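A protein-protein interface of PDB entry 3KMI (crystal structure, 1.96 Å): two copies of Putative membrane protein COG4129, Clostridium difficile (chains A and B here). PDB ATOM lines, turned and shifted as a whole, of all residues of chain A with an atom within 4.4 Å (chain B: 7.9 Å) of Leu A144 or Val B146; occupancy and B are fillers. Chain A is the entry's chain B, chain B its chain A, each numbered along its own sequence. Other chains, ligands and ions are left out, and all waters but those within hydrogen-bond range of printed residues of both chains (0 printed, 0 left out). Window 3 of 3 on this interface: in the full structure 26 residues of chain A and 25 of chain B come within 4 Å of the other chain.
The backbone NH (N) of Val B146 lies within hydrogen-bond range of the side-chain carboxylate (OE1) of Glu B150 (2.8 Å). OD1 of Asp B147 is in hydrogen-bond range of N of Thr B149 (3.3 Å). The backbone NH (N) of Glu B150 lies within hydrogen-bond range of the side-chain carboxylate (OD1) of Asp B147, at 2.8 Å. The backbone carbonyl oxygen (O) of Pro A143 lies within hydrogen-bond range of the guanidinium group (NH2) of Arg A154, 2.6 Å away.
Among the printed residues, pairs that only touch across the chains: Leu A144 with Val B146, Val A146 with Leu B144, Leu A144 with Asp B147, Arg A154 with Phe B151 and Pro A145 with Leu B144.
Gln A142 touches none of the printed residues of chain B. Printed residues of chain B within 4 Å of Leu A144: Val B146 (3.3 Å) and Asp B147 (3.7 Å). Of the printed residues of chain B, Pro A145 touches Leu B144. Printed residues of chain B within 4 Å of Val A146: Leu B144 (3.5 Å). Of the printed residues of chain A, Leu B144 touches Pro A145 (3.7 Å) and Val A146 (3.5 Å). Val B146 touches one residue of chain A. Printed residues of chain A within 4 Å of Asp B147: Leu A144. Of the printed residues of chain A, Phe B151 touches Arg A154. The nearest printed residue of chain A that does not touch Leu B144 is Leu A144 (7.2 Å).
Of the 6 printed residues of chain A, 4 touch a printed residue of chain B. Hydrophobic or aromatic side chains of chain A that line the printed part of chain B: Leu A144. Among the printed residues, no Asp or Glu carboxylate lies within 4 Å of a Lys or Arg side-chain nitrogen of the other chain.
Leu A144 touches Val B146, and with the chains exchanged Val A146 touches Leu B144. Pro A145 touches Leu B144, but with the chains exchanged Leu A144 does not touch Pro B145 (4.04 Å). 5 positions are printed for both chains. Of the 5 pairs that touch across the chains among the printed residues, 2 have their exchanged pair printed and touching as well.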
ATOM      1  N   GLN A 142     -27.690   6.863 -11.241  1.00  0.00           N
ATOM      2  CA  GLN A 142     -27.957   8.113 -11.942  1.00  0.00           C
ATOM      3  C   GLN A 142     -27.099   9.251 -11.379  1.00  0.00           C
ATOM      4  O   GLN A 142     -26.795   9.260 -10.180  1.00  0.00           O
ATOM      5  CB  GLN A 142     -29.430   8.499 -11.796  1.00  0.00           C
ATOM      6  CG  GLN A 142     -30.374   7.812 -12.742  1.00  0.00           C
ATOM      7  CD  GLN A 142     -31.800   8.312 -12.581  1.00  0.00           C
ATOM      8  OE1 GLN A 142     -32.486   7.974 -11.615  1.00  0.00           O
ATOM      9  NE2 GLN A 142     -32.259   9.110 -13.540  1.00  0.00           N
ATOM     10  N   PRO A 143     -26.706  10.217 -12.238  1.00  0.00           N
ATOM     11  CA  PRO A 143     -25.962  11.380 -11.759  1.00  0.00           C
ATOM     12  C   PRO A 143     -26.830  12.231 -10.844  1.00  0.00           C
ATOM     13  O   PRO A 143     -28.044  12.307 -11.039  1.00  0.00           O
ATOM     14  CB  PRO A 143     -25.649  12.160 -13.042  1.00  0.00           C
ATOM     15  CG  PRO A 143     -25.919  11.231 -14.153  1.00  0.00           C
ATOM     16  CD  PRO A 143     -26.970  10.300 -13.684  1.00  0.00           C
ATOM     17  N   LEU A 144     -26.213  12.861  -9.858  1.00  0.00           N
ATOM     18  CA  LEU A 144     -26.925  13.717  -8.907  1.00  0.00           C
ATOM     19  C   LEU A 144     -27.976  14.615  -9.582  1.00  0.00           C
ATOM     20  O   LEU A 144     -27.765  15.081 -10.698  1.00  0.00           O
ATOM     21  CB  LEU A 144     -25.920  14.574  -8.130  1.00  0.00           C
ATOM     22  CG  LEU A 144     -25.106  13.891  -7.027  1.00  0.00           C
ATOM     23  CD1 LEU A 144     -23.761  14.572  -6.817  1.00  0.00           C
ATOM     24  CD2 LEU A 144     -25.898  13.845  -5.726  1.00  0.00           C
ATOM     25  N   PRO A 145     -29.105  14.860  -8.901  1.00  0.00           N
ATOM     26  CA  PRO A 145     -30.155  15.737  -9.430  1.00  0.00           C
ATOM     27  C   PRO A 145     -29.706  17.200  -9.554  1.00  0.00           C
ATOM     28  O   PRO A 145     -29.457  17.870  -8.544  1.00  0.00           O
ATOM     29  CB  PRO A 145     -31.271  15.620  -8.391  1.00  0.00           C
ATOM     30  CG  PRO A 145     -30.938  14.418  -7.556  1.00  0.00           C
ATOM     31  CD  PRO A 145     -29.461  14.299  -7.582  1.00  0.00           C
ATOM     32  N   VAL A 146     -29.609  17.683 -10.788  1.00  0.00           N
ATOM     33  CA  VAL A 146     -29.144  19.042 -11.063  1.00  0.00           C
ATOM     34  C   VAL A 146     -30.180  20.086 -10.651  1.00  0.00           C
ATOM     35  O   VAL A 146     -29.935  20.911  -9.781  1.00  0.00           O
ATOM     36  CB  VAL A 146     -28.781  19.189 -12.535  1.00  0.00           C
ATOM     37  N   ARG A 154     -36.742  12.744  -8.261  1.00  0.00           N
ATOM     38  CA  ARG A 154     -35.826  11.703  -7.793  1.00  0.00           C
ATOM     39  C   ARG A 154     -36.116  11.249  -6.351  1.00  0.00           C
ATOM     40  O   ARG A 154     -36.093  10.036  -6.065  1.00  0.00           O
ATOM     41  CB  ARG A 154     -34.380  12.199  -7.889  1.00  0.00           C
ATOM     42  CG  ARG A 154     -33.303  11.111  -7.680  1.00  0.00           C
ATOM     43  CD  ARG A 154     -33.024  10.316  -8.969  1.00  0.00           C
ATOM     44  NE  ARG A 154     -32.376  11.148  -9.996  1.00  0.00           N
ATOM     45  CZ  ARG A 154     -31.063  11.326 -10.118  1.00  0.00           C
ATOM     46  NH1 ARG A 154     -30.211  10.749  -9.279  1.00  0.00           N
ATOM     47  NH2 ARG A 154     -30.593  12.097 -11.084  1.00  0.00           N
ATOM     48  N   PRO B 143     -31.093  23.288   0.914  1.00  0.00           N
ATOM     49  CA  PRO B 143     -30.079  23.079  -0.132  1.00  0.00           C
ATOM     50  C   PRO B 143     -30.020  21.630  -0.604  1.00  0.00           C
ATOM     51  O   PRO B 143     -30.023  20.721   0.220  1.00  0.00           O
ATOM     52  CB  PRO B 143     -28.776  23.422   0.585  1.00  0.00           C
ATOM     53  CG  PRO B 143     -29.166  24.499   1.541  1.00  0.00           C
ATOM     54  CD  PRO B 143     -30.599  24.217   1.952  1.00  0.00           C
ATOM     55  N   LEU B 144     -29.964  21.443  -1.922  1.00  0.00           N
ATOM     56  CA  LEU B 144     -29.876  20.119  -2.547  1.00  0.00           C
ATOM     57  C   LEU B 144     -28.682  19.322  -2.005  1.00  0.00           C
ATOM     58  O   LEU B 144     -27.705  19.922  -1.552  1.00  0.00           O
ATOM     59  CB  LEU B 144     -29.784  20.253  -4.076  1.00  0.00           C
ATOM     60  CG  LEU B 144     -31.084  20.424  -4.873  1.00  0.00           C
ATOM     61  CD1 LEU B 144     -31.880  21.628  -4.395  1.00  0.00           C
ATOM     62  CD2 LEU B 144     -30.792  20.533  -6.361  1.00  0.00           C
ATOM     63  N   PRO B 145     -28.765  17.974  -2.031  1.00  0.00           N
ATOM     64  CA  PRO B 145     -27.654  17.143  -1.528  1.00  0.00           C
ATOM     65  C   PRO B 145     -26.401  17.224  -2.391  1.00  0.00           C
ATOM     66  O   PRO B 145     -26.496  17.234  -3.610  1.00  0.00           O
ATOM     67  CB  PRO B 145     -28.223  15.710  -1.575  1.00  0.00           C
ATOM     68  CG  PRO B 145     -29.678  15.864  -1.707  1.00  0.00           C
ATOM     69  CD  PRO B 145     -29.884  17.120  -2.477  1.00  0.00           C
ATOM     70  N   VAL B 146     -25.242  17.274  -1.739  1.00  0.00           N
ATOM     71  CA  VAL B 146     -23.934  17.405  -2.404  1.00  0.00           C
ATOM     72  C   VAL B 146     -23.510  16.055  -2.991  1.00  0.00           C
ATOM     73  O   VAL B 146     -22.818  16.004  -4.016  1.00  0.00           O
ATOM     74  CB  VAL B 146     -22.848  17.904  -1.414  1.00  0.00           C
ATOM     75  CG1 VAL B 146     -21.516  18.108  -2.116  1.00  0.00           C
ATOM     76  CG2 VAL B 146     -23.285  19.201  -0.734  1.00  0.00           C
ATOM     77  N   ASP B 147     -23.924  14.971  -2.333  1.00  0.00           N
ATOM     78  CA  ASP B 147     -23.587  13.615  -2.768  1.00  0.00           C
ATOM     79  C   ASP B 147     -24.683  12.579  -2.520  1.00  0.00           C
ATOM     80  O   ASP B 147     -25.762  12.910  -2.004  1.00  0.00           O
ATOM     81  CB  ASP B 147     -22.222  13.151  -2.204  1.00  0.00           C
ATOM     82  CG  ASP B 147     -22.183  13.048  -0.680  1.00  0.00           C
ATOM     83  OD1 ASP B 147     -23.207  12.815  -0.008  1.00  0.00           O
ATOM     84  OD2 ASP B 147     -21.076  13.188  -0.140  1.00  0.00           O
ATOM     85  N   ARG B 148     -24.401  11.328  -2.896  1.00  0.00           N
ATOM     86  CA  ARG B 148     -25.329  10.208  -2.730  1.00  0.00           C
ATOM     87  C   ARG B 148     -25.616   9.910  -1.266  1.00  0.00           C
ATOM     88  O   ARG B 148     -26.769   9.696  -0.884  1.00  0.00           O
ATOM     89  CB  ARG B 148     -24.788   8.949  -3.411  1.00  0.00           C
ATOM     90  CG  ARG B 148     -25.454   7.662  -2.928  1.00  0.00           C
ATOM     91  CD  ARG B 148     -24.879   6.436  -3.632  1.00  0.00           C
ATOM     92  NE  ARG B 148     -25.350   5.172  -3.061  1.00  0.00           N
ATOM     93  CZ  ARG B 148     -24.897   4.646  -1.926  1.00  0.00           C
ATOM     94  NH1 ARG B 148     -23.972   5.279  -1.208  1.00  0.00           N
ATOM     95  NH2 ARG B 148     -25.379   3.484  -1.499  1.00  0.00           N
ATOM     96  N   THR B 149     -24.566   9.891  -0.449  1.00  0.00           N
ATOM     97  CA  THR B 149     -24.730   9.662   0.983  1.00  0.00           C
ATOM     98  C   THR B 149     -25.709  10.667   1.574  1.00  0.00           C
ATOM     99  O   THR B 149     -26.591  10.303   2.343  1.00  0.00           O
ATOM    100  CB  THR B 149     -23.387   9.753   1.737  1.00  0.00           C
ATOM    101  OG1 THR B 149     -22.444   8.853   1.146  1.00  0.00           O
ATOM    102  CG2 THR B 149     -23.574   9.400   3.212  1.00  0.00           C
ATOM    103  N   GLU B 150     -25.551  11.932   1.196  1.00  0.00           N
ATOM    104  CA  GLU B 150     -26.406  13.008   1.685  1.00  0.00           C
ATOM    105  C   GLU B 150     -27.842  12.838   1.192  1.00  0.00           C
ATOM    106  O   GLU B 150     -28.777  12.958   1.970  1.00  0.00           O
ATOM    107  CB  GLU B 150     -25.851  14.331   1.219  1.00  0.00           C
ATOM    108  CG  GLU B 150     -26.343  15.565   1.939  1.00  0.00           C
ATOM    109  CD  GLU B 150     -25.572  16.786   1.457  1.00  0.00           C
ATOM    110  OE1 GLU B 150     -24.491  16.589   0.860  1.00  0.00           O
ATOM    111  OE2 GLU B 150     -26.027  17.937   1.651  1.00  0.00           O
ATOM    112  N   PHE B 151     -28.004  12.554  -0.096  1.00  0.00           N
ATOM    113  CA  PHE B 151     -29.324  12.249  -0.662  1.00  0.00           C
ATOM    114  C   PHE B 151     -30.029  11.153   0.140  1.00  0.00           C
ATOM    115  O   PHE B 151     -31.186  11.316   0.547  1.00  0.00           O
ATOM    116  CB  PHE B 151     -29.191  11.855  -2.138  1.00  0.00           C
ATOM    117  CG  PHE B 151     -30.491  11.477  -2.796  1.00  0.00           C
ATOM    118  CD1 PHE B 151     -31.259  12.439  -3.459  1.00  0.00           C
ATOM    119  CD2 PHE B 151     -30.927  10.142  -2.788  1.00  0.00           C
ATOM    120  CE1 PHE B 151     -32.461  12.069  -4.108  1.00  0.00           C
ATOM    121  CE2 PHE B 151     -32.107   9.770  -3.398  1.00  0.00           C
ATOM    122  CZ  PHE B 151     -32.880  10.727  -4.068  1.00  0.00           C
ATOM    123  N   ARG B 154     -31.101  12.084   3.795  1.00  0.00           N
ATOM    124  CA  ARG B 154     -32.251  12.967   3.745  1.00  0.00           C
ATOM    125  C   ARG B 154     -33.516  12.174   3.508  1.00  0.00           C
ATOM    126  O   ARG B 154     -34.498  12.342   4.241  1.00  0.00           O
ATOM    127  CB  ARG B 154     -32.057  14.011   2.642  1.00  0.00           C
ATOM    128  CG  ARG B 154     -30.915  14.951   2.929  1.00  0.00           C
ATOM    129  CD  ARG B 154     -31.407  16.327   3.274  1.00  0.00           C
ATOM    130  NE  ARG B 154     -31.670  17.158   2.101  1.00  0.00           N
ATOM    131  CZ  ARG B 154     -32.886  17.402   1.627  1.00  0.00           C
ATOM    132  NH1 ARG B 154     -33.947  16.874   2.228  1.00  0.00           N
ATOM    133  NH2 ARG B 154     -33.040  18.174   0.561  1.00  0.00           N
